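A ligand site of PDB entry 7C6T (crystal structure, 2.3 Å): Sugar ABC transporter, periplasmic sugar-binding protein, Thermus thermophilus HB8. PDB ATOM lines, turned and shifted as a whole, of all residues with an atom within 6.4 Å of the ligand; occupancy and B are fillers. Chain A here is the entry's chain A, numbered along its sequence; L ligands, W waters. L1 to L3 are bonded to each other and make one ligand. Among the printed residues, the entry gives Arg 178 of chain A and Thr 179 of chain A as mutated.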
ATOM      1  N   PRO A  11     -25.191  25.038 -13.153  1.00  0.00           N
ATOM      2  CA  PRO A  11     -24.496  24.471 -14.318  1.00  0.00           C
ATOM      3  C   PRO A  11     -23.913  23.105 -13.951  1.00  0.00           C
ATOM      4  O   PRO A  11     -22.702  23.043 -13.704  1.00  0.00           O
ATOM      5  CB  PRO A  11     -23.352  25.453 -14.585  1.00  0.00           C
ATOM      6  CG  PRO A  11     -23.847  26.710 -13.891  1.00  0.00           C
ATOM      7  CD  PRO A  11     -24.425  26.161 -12.601  1.00  0.00           C
ATOM      8  N   ASN A  12     -24.729  22.055 -13.940  1.00  0.00           N
ATOM      9  CA  ASN A  12     -24.323  20.786 -13.311  1.00  0.00           C
ATOM     10  C   ASN A  12     -23.519  19.921 -14.286  1.00  0.00           C
ATOM     11  O   ASN A  12     -22.997  18.925 -13.848  1.00  0.00           O
ATOM     12  CB  ASN A  12     -25.535  20.042 -12.778  1.00  0.00           C
ATOM     13  CG  ASN A  12     -26.348  20.791 -11.754  1.00  0.00           C
ATOM     14  OD1 ASN A  12     -25.790  21.275 -10.760  1.00  0.00           O
ATOM     15  ND2 ASN A  12     -27.685  20.793 -11.923  1.00  0.00           N
ATOM     16  N   SER A  13     -23.498  20.241 -15.577  1.00  0.00           N
ATOM     17  CA  SER A  13     -22.884  19.449 -16.652  1.00  0.00           C
ATOM     18  C   SER A  13     -22.373  20.422 -17.702  1.00  0.00           C
ATOM     19  O   SER A  13     -22.800  21.569 -17.730  1.00  0.00           O
ATOM     20  CB  SER A  13     -23.877  18.433 -17.216  1.00  0.00           C
ATOM     21  OG  SER A  13     -25.116  18.979 -17.656  1.00  0.00           O
ATOM     22  N   PRO A  14     -21.454  20.028 -18.599  1.00  0.00           N
ATOM     23  CA  PRO A  14     -20.943  20.946 -19.614  1.00  0.00           C
ATOM     24  C   PRO A  14     -22.028  21.687 -20.429  1.00  0.00           C
ATOM     25  O   PRO A  14     -21.897  22.915 -20.571  1.00  0.00           O
ATOM     26  CB  PRO A  14     -20.121  20.021 -20.517  1.00  0.00           C
ATOM     27  CG  PRO A  14     -19.729  18.851 -19.635  1.00  0.00           C
ATOM     28  CD  PRO A  14     -20.920  18.653 -18.733  1.00  0.00           C
ATOM     29  N   TRP A  42     -23.493  29.273 -10.131  1.00  0.00           N
ATOM     30  CA  TRP A  42     -23.269  29.130  -8.674  1.00  0.00           C
ATOM     31  C   TRP A  42     -22.923  30.489  -8.017  1.00  0.00           C
ATOM     32  O   TRP A  42     -23.495  30.795  -6.923  1.00  0.00           O
ATOM     33  CB  TRP A  42     -22.199  28.058  -8.413  1.00  0.00           C
ATOM     34  CG  TRP A  42     -22.723  26.651  -8.497  1.00  0.00           C
ATOM     35  CD1 TRP A  42     -22.470  25.711  -9.459  1.00  0.00           C
ATOM     36  CD2 TRP A  42     -23.547  25.997  -7.529  1.00  0.00           C
ATOM     37  NE1 TRP A  42     -23.040  24.520  -9.130  1.00  0.00           N
ATOM     38  CE2 TRP A  42     -23.727  24.663  -7.965  1.00  0.00           C
ATOM     39  CE3 TRP A  42     -24.150  26.412  -6.334  1.00  0.00           C
ATOM     40  CZ2 TRP A  42     -24.493  23.749  -7.254  1.00  0.00           C
ATOM     41  CZ3 TRP A  42     -24.936  25.521  -5.653  1.00  0.00           C
ATOM     42  CH2 TRP A  42     -25.094  24.200  -6.105  1.00  0.00           C
ATOM     43  N   GLY A  43     -22.143  31.346  -8.695  1.00  0.00           N
ATOM     44  CA  GLY A  43     -21.754  32.679  -8.171  1.00  0.00           C
ATOM     45  C   GLY A  43     -22.977  33.553  -7.868  1.00  0.00           C
ATOM     46  O   GLY A  43     -22.876  34.457  -6.983  1.00  0.00           O
ATOM     47  N   LEU A  64     -31.401  23.608  -5.119  1.00  0.00           N
ATOM     48  CA  LEU A  64     -30.708  24.162  -3.933  1.00  0.00           C
ATOM     49  C   LEU A  64     -29.475  23.304  -3.613  1.00  0.00           C
ATOM     50  O   LEU A  64     -29.636  22.046  -3.518  1.00  0.00           O
ATOM     51  CB  LEU A  64     -31.675  24.066  -2.782  1.00  0.00           C
ATOM     52  CG  LEU A  64     -32.914  24.903  -2.858  1.00  0.00           C
ATOM     53  CD1 LEU A  64     -33.683  24.760  -1.577  1.00  0.00           C
ATOM     54  CD2 LEU A  64     -32.563  26.364  -3.075  1.00  0.00           C
ATOM     55  N   GLY A  65     -28.363  23.951  -3.308  1.00  0.00           N
ATOM     56  CA  GLY A  65     -27.335  23.401  -2.443  1.00  0.00           C
ATOM     57  C   GLY A  65     -27.954  22.801  -1.194  1.00  0.00           C
ATOM     58  O   GLY A  65     -28.847  23.494  -0.598  1.00  0.00           O
ATOM     59  N   THR A  66     -27.523  21.581  -0.797  1.00  0.00           N
ATOM     60  CA  THR A  66     -27.962  20.936   0.463  1.00  0.00           C
ATOM     61  C   THR A  66     -27.788  21.932   1.601  1.00  0.00           C
ATOM     62  O   THR A  66     -28.662  22.009   2.465  1.00  0.00           O
ATOM     63  CB  THR A  66     -27.192  19.640   0.768  1.00  0.00           C
ATOM     64  OG1 THR A  66     -25.783  19.868   0.724  1.00  0.00           O
ATOM     65  CG2 THR A  66     -27.497  18.501  -0.192  1.00  0.00           C
ATOM     66  N   THR A  67     -26.738  22.735   1.615  1.00  0.00           N
ATOM     67  CA  THR A  67     -26.481  23.626   2.771  1.00  0.00           C
ATOM     68  C   THR A  67     -27.346  24.886   2.704  1.00  0.00           C
ATOM     69  O   THR A  67     -27.318  25.628   3.718  1.00  0.00           O
ATOM     70  CB  THR A  67     -25.020  24.039   2.890  1.00  0.00           C
ATOM     71  OG1 THR A  67     -24.727  24.953   1.846  1.00  0.00           O
ATOM     72  CG2 THR A  67     -24.112  22.846   2.823  1.00  0.00           C
ATOM     73  N   TRP A  68     -28.141  25.104   1.658  1.00  0.00           N
ATOM     74  CA  TRP A  68     -29.087  26.256   1.621  1.00  0.00           C
ATOM     75  C   TRP A  68     -30.512  25.940   2.090  1.00  0.00           C
ATOM     76  O   TRP A  68     -31.259  26.900   2.146  1.00  0.00           O
ATOM     77  CB  TRP A  68     -29.218  26.794   0.206  1.00  0.00           C
ATOM     78  CG  TRP A  68     -27.918  27.185  -0.365  1.00  0.00           C
ATOM     79  CD1 TRP A  68     -26.741  27.365   0.297  1.00  0.00           C
ATOM     80  CD2 TRP A  68     -27.726  27.571  -1.723  1.00  0.00           C
ATOM     81  NE1 TRP A  68     -25.790  27.797  -0.590  1.00  0.00           N
ATOM     82  CE2 TRP A  68     -26.372  27.894  -1.848  1.00  0.00           C
ATOM     83  CE3 TRP A  68     -28.575  27.632  -2.836  1.00  0.00           C
ATOM     84  CZ2 TRP A  68     -25.834  28.335  -3.050  1.00  0.00           C
ATOM     85  CZ3 TRP A  68     -28.052  28.064  -4.028  1.00  0.00           C
ATOM     86  CH2 TRP A  68     -26.698  28.419  -4.128  1.00  0.00           C
ATOM     87  N   PHE A 116     -28.941  14.931  -6.262  1.00  0.00           N
ATOM     88  CA  PHE A 116     -27.633  14.273  -6.502  1.00  0.00           C
ATOM     89  C   PHE A 116     -26.714  14.646  -5.347  1.00  0.00           C
ATOM     90  O   PHE A 116     -26.981  15.607  -4.600  1.00  0.00           O
ATOM     91  CB  PHE A 116     -27.073  14.664  -7.867  1.00  0.00           C
ATOM     92  CG  PHE A 116     -26.776  16.141  -8.072  1.00  0.00           C
ATOM     93  CD1 PHE A 116     -25.613  16.705  -7.587  1.00  0.00           C
ATOM     94  CD2 PHE A 116     -27.613  16.956  -8.818  1.00  0.00           C
ATOM     95  CE1 PHE A 116     -25.279  18.032  -7.819  1.00  0.00           C
ATOM     96  CE2 PHE A 116     -27.288  18.294  -9.017  1.00  0.00           C
ATOM     97  CZ  PHE A 116     -26.098  18.821  -8.560  1.00  0.00           C
ATOM     98  N   GLU A 118     -22.523  14.871  -3.973  1.00  0.00           N
ATOM     99  CA  GLU A 118     -21.106  15.022  -4.299  1.00  0.00           C
ATOM    100  C   GLU A 118     -20.360  14.976  -2.975  1.00  0.00           C
ATOM    101  O   GLU A 118     -20.974  15.322  -1.946  1.00  0.00           O
ATOM    102  CB  GLU A 118     -20.927  16.254  -5.175  1.00  0.00           C
ATOM    103  CG  GLU A 118     -21.236  17.605  -4.525  1.00  0.00           C
ATOM    104  CD  GLU A 118     -19.974  18.364  -4.108  1.00  0.00           C
ATOM    105  OE1 GLU A 118     -20.037  19.615  -3.933  1.00  0.00           O
ATOM    106  OE2 GLU A 118     -18.911  17.696  -3.977  1.00  0.00           O
ATOM    107  N   ARG A 120     -15.857  15.181  -1.535  1.00  0.00           N
ATOM    108  CA  ARG A 120     -14.524  15.674  -1.920  1.00  0.00           C
ATOM    109  C   ARG A 120     -13.475  14.612  -1.585  1.00  0.00           C
ATOM    110  O   ARG A 120     -13.576  13.889  -0.613  1.00  0.00           O
ATOM    111  CB  ARG A 120     -14.230  17.038  -1.296  1.00  0.00           C
ATOM    112  CG  ARG A 120     -15.358  18.029  -1.474  1.00  0.00           C
ATOM    113  CD  ARG A 120     -15.630  18.377  -2.895  1.00  0.00           C
ATOM    114  NE  ARG A 120     -16.828  19.200  -3.154  1.00  0.00           N
ATOM    115  CZ  ARG A 120     -16.862  20.540  -3.154  1.00  0.00           C
ATOM    116  NH1 ARG A 120     -15.784  21.215  -2.799  1.00  0.00           N
ATOM    117  NH2 ARG A 120     -18.000  21.189  -3.465  1.00  0.00           N
ATOM    118  N   ARG A 178     -15.506  30.878  -0.803  1.00  0.00           N
ATOM    119  CA  ARG A 178     -16.969  31.111  -0.700  1.00  0.00           C
ATOM    120  C   ARG A 178     -17.512  30.273   0.468  1.00  0.00           C
ATOM    121  O   ARG A 178     -18.474  30.724   1.059  1.00  0.00           O
ATOM    122  CB  ARG A 178     -17.603  30.822  -2.071  1.00  0.00           C
ATOM    123  CG  ARG A 178     -18.673  31.824  -2.445  1.00  0.00           C
ATOM    124  CD  ARG A 178     -18.525  32.243  -3.900  1.00  0.00           C
ATOM    125  NE  ARG A 178     -18.482  31.086  -4.777  1.00  0.00           N
ATOM    126  CZ  ARG A 178     -18.337  31.162  -6.087  1.00  0.00           C
ATOM    127  NH1 ARG A 178     -18.339  30.047  -6.803  1.00  0.00           N
ATOM    128  NH2 ARG A 178     -18.198  32.354  -6.667  1.00  0.00           N
ATOM    129  N   THR A 179     -16.851  29.158   0.817  1.00  0.00           N
ATOM    130  CA  THR A 179     -17.336  28.161   1.788  1.00  0.00           C
ATOM    131  C   THR A 179     -16.145  27.535   2.520  1.00  0.00           C
ATOM    132  O   THR A 179     -15.031  27.630   2.042  1.00  0.00           O
ATOM    133  CB  THR A 179     -18.175  27.054   1.106  1.00  0.00           C
ATOM    134  OG1 THR A 179     -17.275  26.212   0.382  1.00  0.00           O
ATOM    135  CG2 THR A 179     -19.185  27.564   0.099  1.00  0.00           C
ATOM    136  N   HIS A 181     -15.845  24.302   2.474  1.00  0.00           N
ATOM    137  CA  HIS A 181     -15.751  22.926   1.879  1.00  0.00           C
ATOM    138  C   HIS A 181     -14.287  22.429   1.894  1.00  0.00           C
ATOM    139  O   HIS A 181     -14.110  21.323   2.383  1.00  0.00           O
ATOM    140  CB  HIS A 181     -16.455  22.773   0.515  1.00  0.00           C
ATOM    141  CG  HIS A 181     -17.879  23.202   0.523  1.00  0.00           C
ATOM    142  ND1 HIS A 181     -18.530  23.520  -0.641  1.00  0.00           N
ATOM    143  CD2 HIS A 181     -18.742  23.431   1.561  1.00  0.00           C
ATOM    144  CE1 HIS A 181     -19.740  23.959  -0.317  1.00  0.00           C
ATOM    145  NE2 HIS A 181     -19.907  23.856   1.033  1.00  0.00           N
ATOM    146  N   THR A 236     -11.271  28.559  -6.507  1.00  0.00           N
ATOM    147  CA  THR A 236     -11.460  27.102  -6.784  1.00  0.00           C
ATOM    148  C   THR A 236     -11.261  26.904  -8.271  1.00  0.00           C
ATOM    149  O   THR A 236     -10.489  26.030  -8.646  1.00  0.00           O
ATOM    150  CB  THR A 236     -12.782  26.580  -6.215  1.00  0.00           C
ATOM    151  OG1 THR A 236     -12.591  26.604  -4.786  1.00  0.00           O
ATOM    152  CG2 THR A 236     -13.149  25.156  -6.626  1.00  0.00           C
ATOM    153  N   ALA A 237     -11.939  27.677  -9.111  1.00  0.00           N
ATOM    154  CA  ALA A 237     -12.016  27.408 -10.570  1.00  0.00           C
ATOM    155  C   ALA A 237     -10.623  27.484 -11.200  1.00  0.00           C
ATOM    156  O   ALA A 237     -10.308  26.730 -12.135  1.00  0.00           O
ATOM    157  CB  ALA A 237     -12.967  28.397 -11.226  1.00  0.00           C
ATOM    158  N   GLU A 240      -8.617  24.422 -10.255  1.00  0.00           N
ATOM    159  CA  GLU A 240      -9.095  23.350 -11.180  1.00  0.00           C
ATOM    160  C   GLU A 240      -8.315  23.446 -12.503  1.00  0.00           C
ATOM    161  O   GLU A 240      -7.686  22.431 -12.926  1.00  0.00           O
ATOM    162  CB  GLU A 240     -10.600  23.423 -11.438  1.00  0.00           C
ATOM    163  CG  GLU A 240     -11.470  22.923 -10.297  1.00  0.00           C
ATOM    164  CD  GLU A 240     -12.978  22.936 -10.570  1.00  0.00           C
ATOM    165  OE1 GLU A 240     -13.364  22.889 -11.776  1.00  0.00           O
ATOM    166  OE2 GLU A 240     -13.784  22.974  -9.582  1.00  0.00           O
ATOM    167  N   TRP A 256     -16.945  15.388 -10.354  1.00  0.00           N
ATOM    168  CA  TRP A 256     -17.219  15.870 -11.730  1.00  0.00           C
ATOM    169  C   TRP A 256     -15.945  15.659 -12.529  1.00  0.00           C
ATOM    170  O   TRP A 256     -16.059  15.244 -13.696  1.00  0.00           O
ATOM    171  CB  TRP A 256     -17.724  17.302 -11.796  1.00  0.00           C
ATOM    172  CG  TRP A 256     -16.957  18.258 -10.971  1.00  0.00           C
ATOM    173  CD1 TRP A 256     -15.934  19.048 -11.353  1.00  0.00           C
ATOM    174  CD2 TRP A 256     -17.184  18.551  -9.584  1.00  0.00           C
ATOM    175  NE1 TRP A 256     -15.516  19.836 -10.319  1.00  0.00           N
ATOM    176  CE2 TRP A 256     -16.293  19.569  -9.224  1.00  0.00           C
ATOM    177  CE3 TRP A 256     -18.122  18.124  -8.636  1.00  0.00           C
ATOM    178  CZ2 TRP A 256     -16.261  20.126  -7.947  1.00  0.00           C
ATOM    179  CZ3 TRP A 256     -18.105  18.688  -7.375  1.00  0.00           C
ATOM    180  CH2 TRP A 256     -17.147  19.630  -7.019  1.00  0.00           C
ATOM    181  N   ARG A 260     -15.144  14.943 -16.696  1.00  0.00           N
ATOM    182  CA  ARG A 260     -14.420  16.003 -17.428  1.00  0.00           C
ATOM    183  C   ARG A 260     -13.138  15.401 -18.028  1.00  0.00           C
ATOM    184  O   ARG A 260     -12.817  15.738 -19.201  1.00  0.00           O
ATOM    185  CB  ARG A 260     -14.129  17.215 -16.526  1.00  0.00           C
ATOM    186  CG  ARG A 260     -14.552  18.563 -17.099  1.00  0.00           C
ATOM    187  CD  ARG A 260     -15.926  19.070 -16.651  1.00  0.00           C
ATOM    188  NE  ARG A 260     -16.947  18.031 -16.522  1.00  0.00           N
ATOM    189  CZ  ARG A 260     -18.089  18.124 -15.799  1.00  0.00           C
ATOM    190  NH1 ARG A 260     -18.395  19.235 -15.144  1.00  0.00           N
ATOM    191  NH2 ARG A 260     -18.927  17.094 -15.747  1.00  0.00           N
ATOM    192  N   GLY A 268     -15.505  21.156 -22.999  1.00  0.00           N
ATOM    193  CA  GLY A 268     -15.445  21.601 -21.578  1.00  0.00           C
ATOM    194  C   GLY A 268     -14.640  20.627 -20.717  1.00  0.00           C
ATOM    195  O   GLY A 268     -14.926  20.524 -19.498  1.00  0.00           O
ATOM    196  N   PHE A 294     -16.010  16.428   3.141  1.00  0.00           N
ATOM    197  CA  PHE A 294     -17.276  17.165   3.024  1.00  0.00           C
ATOM    198  C   PHE A 294     -18.133  16.329   2.089  1.00  0.00           C
ATOM    199  O   PHE A 294     -17.618  15.888   1.017  1.00  0.00           O
ATOM    200  CB  PHE A 294     -17.063  18.606   2.574  1.00  0.00           C
ATOM    201  CG  PHE A 294     -18.337  19.262   2.169  1.00  0.00           C
ATOM    202  CD1 PHE A 294     -19.232  19.723   3.136  1.00  0.00           C
ATOM    203  CD2 PHE A 294     -18.670  19.376   0.840  1.00  0.00           C
ATOM    204  CE1 PHE A 294     -20.449  20.274   2.767  1.00  0.00           C
ATOM    205  CE2 PHE A 294     -19.854  19.988   0.491  1.00  0.00           C
ATOM    206  CZ  PHE A 294     -20.742  20.411   1.436  1.00  0.00           C
ATOM    207  N   PHE A 295     -19.381  16.140   2.530  1.00  0.00           N
ATOM    208  CA  PHE A 295     -20.434  15.450   1.795  1.00  0.00           C
ATOM    209  C   PHE A 295     -21.504  16.484   1.447  1.00  0.00           C
ATOM    210  O   PHE A 295     -22.142  17.040   2.356  1.00  0.00           O
ATOM    211  CB  PHE A 295     -21.100  14.381   2.641  1.00  0.00           C
ATOM    212  CG  PHE A 295     -21.998  13.499   1.822  1.00  0.00           C
ATOM    213  CD1 PHE A 295     -23.322  13.848   1.621  1.00  0.00           C
ATOM    214  CD2 PHE A 295     -21.483  12.389   1.159  1.00  0.00           C
ATOM    215  CE1 PHE A 295     -24.141  13.029   0.850  1.00  0.00           C
ATOM    216  CE2 PHE A 295     -22.298  11.627   0.325  1.00  0.00           C
ATOM    217  CZ  PHE A 295     -23.622  11.947   0.176  1.00  0.00           C
ATOM    218  N   GLY A 296     -21.726  16.721   0.163  1.00  0.00           N
ATOM    219  CA  GLY A 296     -22.802  17.625  -0.259  1.00  0.00           C
ATOM    220  C   GLY A 296     -23.648  17.133  -1.423  1.00  0.00           C
ATOM    221  O   GLY A 296     -24.101  15.982  -1.434  1.00  0.00           O
ATOM    222  N   GLY A 297     -24.009  18.111  -2.241  1.00  0.00           N
ATOM    223  CA  GLY A 297     -24.912  17.996  -3.380  1.00  0.00           C
ATOM    224  C   GLY A 297     -26.001  19.046  -3.377  1.00  0.00           C
ATOM    225  O   GLY A 297     -25.868  20.065  -2.703  1.00  0.00           O
ATOM    226  N   SER A 298     -27.093  18.702  -4.066  1.00  0.00           N
ATOM    227  CA  SER A 298     -28.208  19.582  -4.391  1.00  0.00           C
ATOM    228  C   SER A 298     -29.508  18.782  -4.298  1.00  0.00           C
ATOM    229  O   SER A 298     -29.532  17.569  -4.645  1.00  0.00           O
ATOM    230  CB  SER A 298     -28.020  20.170  -5.787  1.00  0.00           C
ATOM    231  OG  SER A 298     -27.000  21.161  -5.821  1.00  0.00           O
ATOM    232  N   THR A 332     -23.858  14.258 -15.397  1.00  0.00           N
ATOM    233  CA  THR A 332     -23.200  15.272 -14.529  1.00  0.00           C
ATOM    234  C   THR A 332     -21.828  14.805 -14.026  1.00  0.00           C
ATOM    235  O   THR A 332     -21.050  15.664 -13.667  1.00  0.00           O
ATOM    236  CB  THR A 332     -24.021  15.711 -13.320  1.00  0.00           C
ATOM    237  OG1 THR A 332     -24.358  14.550 -12.575  1.00  0.00           O
ATOM    238  CG2 THR A 332     -25.304  16.403 -13.728  1.00  0.00           C
ATOM    239  N   MET A 334     -21.843  13.160 -11.223  1.00  0.00           N
ATOM    240  CA  MET A 334     -22.145  13.189  -9.768  1.00  0.00           C
ATOM    241  C   MET A 334     -22.539  11.774  -9.287  1.00  0.00           C
ATOM    242  O   MET A 334     -22.601  10.880 -10.070  1.00  0.00           O
ATOM    243  CB  MET A 334     -23.310  14.154  -9.462  1.00  0.00           C
ATOM    244  CG  MET A 334     -23.069  15.576  -9.888  1.00  0.00           C
ATOM    245  SD  MET A 334     -21.774  16.480  -8.923  1.00  0.00           S
ATOM    246  CE  MET A 334     -21.932  18.039  -9.775  1.00  0.00           C
ATOM    247  N   GLU A 376     -21.297  30.494   7.818  1.00  0.00           N
ATOM    248  CA  GLU A 376     -20.221  30.128   6.863  1.00  0.00           C
ATOM    249  C   GLU A 376     -19.565  31.409   6.344  1.00  0.00           C
ATOM    250  O   GLU A 376     -18.328  31.411   6.238  1.00  0.00           O
ATOM    251  CB  GLU A 376     -20.755  29.239   5.754  1.00  0.00           C
ATOM    252  CG  GLU A 376     -19.658  28.519   4.988  1.00  0.00           C
ATOM    253  CD  GLU A 376     -20.112  27.188   4.372  1.00  0.00           C
ATOM    254  OE1 GLU A 376     -21.353  27.071   3.937  1.00  0.00           O
ATOM    255  OE2 GLU A 376     -19.195  26.268   4.283  1.00  0.00           O
HETATM  256  C1  LIG L   1     -19.868  21.213 -10.782  1.00  0.00           C
HETATM  257  C2  LIG L   1     -19.190  22.411 -10.143  1.00  0.00           C
HETATM  258  C3  LIG L   1     -17.884  22.701 -10.882  1.00  0.00           C
HETATM  259  C4  LIG L   1     -18.180  22.857 -12.375  1.00  0.00           C
HETATM  260  C5  LIG L   1     -17.002  23.166 -13.301  1.00  0.00           C
HETATM  261  C6  LIG L   1     -20.044  21.433 -12.263  1.00  0.00           C
HETATM  262  O1  LIG L   1     -20.616  20.335 -12.959  1.00  0.00           O
HETATM  263  O2  LIG L   1     -21.122  21.094 -10.120  1.00  0.00           O
HETATM  264  O3  LIG L   1     -19.032  22.084  -8.753  1.00  0.00           O
HETATM  265  O4  LIG L   1     -17.302  23.873 -10.305  1.00  0.00           O
HETATM  266  O5  LIG L   1     -18.747  21.621 -12.807  1.00  0.00           O
HETATM  267  O6  LIG L   1     -17.024  22.312 -14.475  1.00  0.00           O
HETATM  268  C1  LG2 L   2     -19.948  22.261  -6.487  1.00  0.00           C
HETATM  269  C2  LG2 L   2     -20.654  23.259  -5.553  1.00  0.00           C
HETATM  270  C3  LG2 L   2     -19.950  24.603  -5.509  1.00  0.00           C
HETATM  271  C4  LG2 L   2     -19.760  25.097  -6.959  1.00  0.00           C
HETATM  272  C5  LG2 L   2     -19.039  26.438  -7.143  1.00  0.00           C
HETATM  273  C6  LG2 L   2     -19.724  22.924  -7.848  1.00  0.00           C
HETATM  274  O1  LG2 L   2     -20.798  21.131  -6.626  1.00  0.00           O
HETATM  275  O2  LG2 L   2     -20.774  22.770  -4.230  1.00  0.00           O
HETATM  276  O3  LG2 L   2     -20.808  25.471  -4.763  1.00  0.00           O
HETATM  277  O4  LG2 L   2     -18.994  24.142  -7.676  1.00  0.00           O
HETATM  278  O5  LG2 L   2     -17.798  26.304  -6.468  1.00  0.00           O
HETATM  279  C1  LG3 L   3     -22.249  21.781  -2.617  1.00  0.00           C
HETATM  280  C2  LG3 L   3     -23.545  21.947  -1.828  1.00  0.00           C
HETATM  281  C3  LG3 L   3     -23.540  23.312  -1.139  1.00  0.00           C
HETATM  282  C4  LG3 L   3     -23.323  24.357  -2.225  1.00  0.00           C
HETATM  283  C5  LG3 L   3     -23.260  25.807  -1.808  1.00  0.00           C
HETATM  284  C6  LG3 L   3     -22.054  22.904  -3.617  1.00  0.00           C
HETATM  285  O1  LG3 L   3     -22.212  20.514  -3.266  1.00  0.00           O
HETATM  286  O2  LG3 L   3     -23.479  20.870  -0.899  1.00  0.00           O
HETATM  287  O3  LG3 L   3     -24.765  23.521  -0.444  1.00  0.00           O
HETATM  288  O4  LG3 L   3     -22.098  24.117  -2.868  1.00  0.00           O
HETATM  289  O5  LG3 L   3     -22.160  26.093  -0.980  1.00  0.00           O
HETATM  290  O   HOH W   1     -21.855  25.299   2.133  1.00  0.00           O
HETATM  291  O   HOH W   2     -22.848  28.501   0.083  1.00  0.00           O
HETATM  292  O   HOH W   3     -24.449  20.512  -5.653  1.00  0.00           O
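An oxygen (O2) of LG3 L3 lies within hydrogen-bond range of the backbone carbonyl oxygen (O) of Gly 297. The backbone carbonyl oxygen (O) of Asn 12 lies within hydrogen-bond range of an oxygen (O1) of LIG L1 (2.9 Å). An oxygen (O1) of LIG L1 is in hydrogen-bond range of the guanidinium group (NH1) of Arg 260 (3.3 Å). The backbone NH of Gly 297 is in hydrogen-bond range of an oxygen (O2) of LG3 L3 (3.1 Å). O3 of LG3 L3 is in hydrogen-bond range of OG1 of Thr 67 (2.7 Å). The guanidinium group (NH2) of Arg 120 sits at hydrogen-bond distance from an oxygen (O2) of LG2 L2 (3.3 Å). An oxygen (O1) of LIG L1 sits close to the backbone carbonyl oxygen (O) of Pro 11. O3 of LG3 L3 sits at hydrogen-bond distance from N of Thr 66 (3.4 Å). An oxygen (O1) of LG3 L3 lies within hydrogen-bond range of the side-chain carboxylate (OE1) of Glu 118 (2.4 Å). The side-chain hydroxyl of Thr 66 sits at hydrogen-bond distance from an oxygen (O2) of LG3 L3. An oxygen (O3) of LG3 L3 is in hydrogen-bond range of the backbone NH of Thr 67 (3.0 Å).
The backbone NH of Met 334 lies close to the side-chain hydroxyl of Thr 332 (3.2 Å). O of Thr 332 is in hydrogen-bond range of NH2 of Arg 260. The backbone carbonyl oxygen of Phe 294 is in hydrogen-bond range of the backbone NH of Arg 120 (3.2 Å). The guanidinium group of Arg 120 is in salt-bridge range of the side-chain carboxylate of Glu 118, 2.6 Å away. The backbone carbonyl oxygen of Glu 118 sits at hydrogen-bond distance from the backbone NH of Gly 296 (2.6 Å). The backbone NH of Thr 66 sits at hydrogen-bond distance from the backbone carbonyl oxygen of Gly 297 (2.9 Å). OG1 of Thr 179 lies close to ND1 of His 181, at 3.1 Å.
N of Ser 13 touches O1 of LIG L1, 3.9 Å away. CG of Trp 42 touches C4 of LG2 L2, at 3.7 Å. CA of Gly 65 touches O3 of LG3 L3 (3.3 Å). Trp 68 touches the ligand. Arg 178 touches the ligand. CG2 of Thr 179 touches O5 of LG3 L3, at 3.5 Å. CE1 of His 181 touches O5 of LG3 L3, 3.3 Å away. OE2 of Glu 240 touches O4 of LIG L1 (3.7 Å). CZ2 of Trp 256 touches O3 of LIG L1 (3.5 Å). CZ of Phe 294 touches O2 of LG3 L3, 3.6 Å away. Gly 296 touches the ligand. CE of Met 334 touches O2 of LIG L1, 3.2 Å away. Of the 31 residues printed, 20 come within 4 Å of the ligand. The nearest printed residue that does not touch the ligand is Thr 332 (4.7 Å).
Water W2 bridges O5 of LG3 L3 (2.7 Å) and NE1 of Trp 68 (3.1 Å). Water W1 lies within hydrogen-bond range of the side-chain carboxylate of Glu 376, a ring nitrogen (NE2) of His 181, the side-chain hydroxyl of Thr 67 and an oxygen (O5) of LG3 L3. Water W3 lies within hydrogen-bond range of OG of Ser 298, O1 of LG3 L3 and O of Gly 297.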
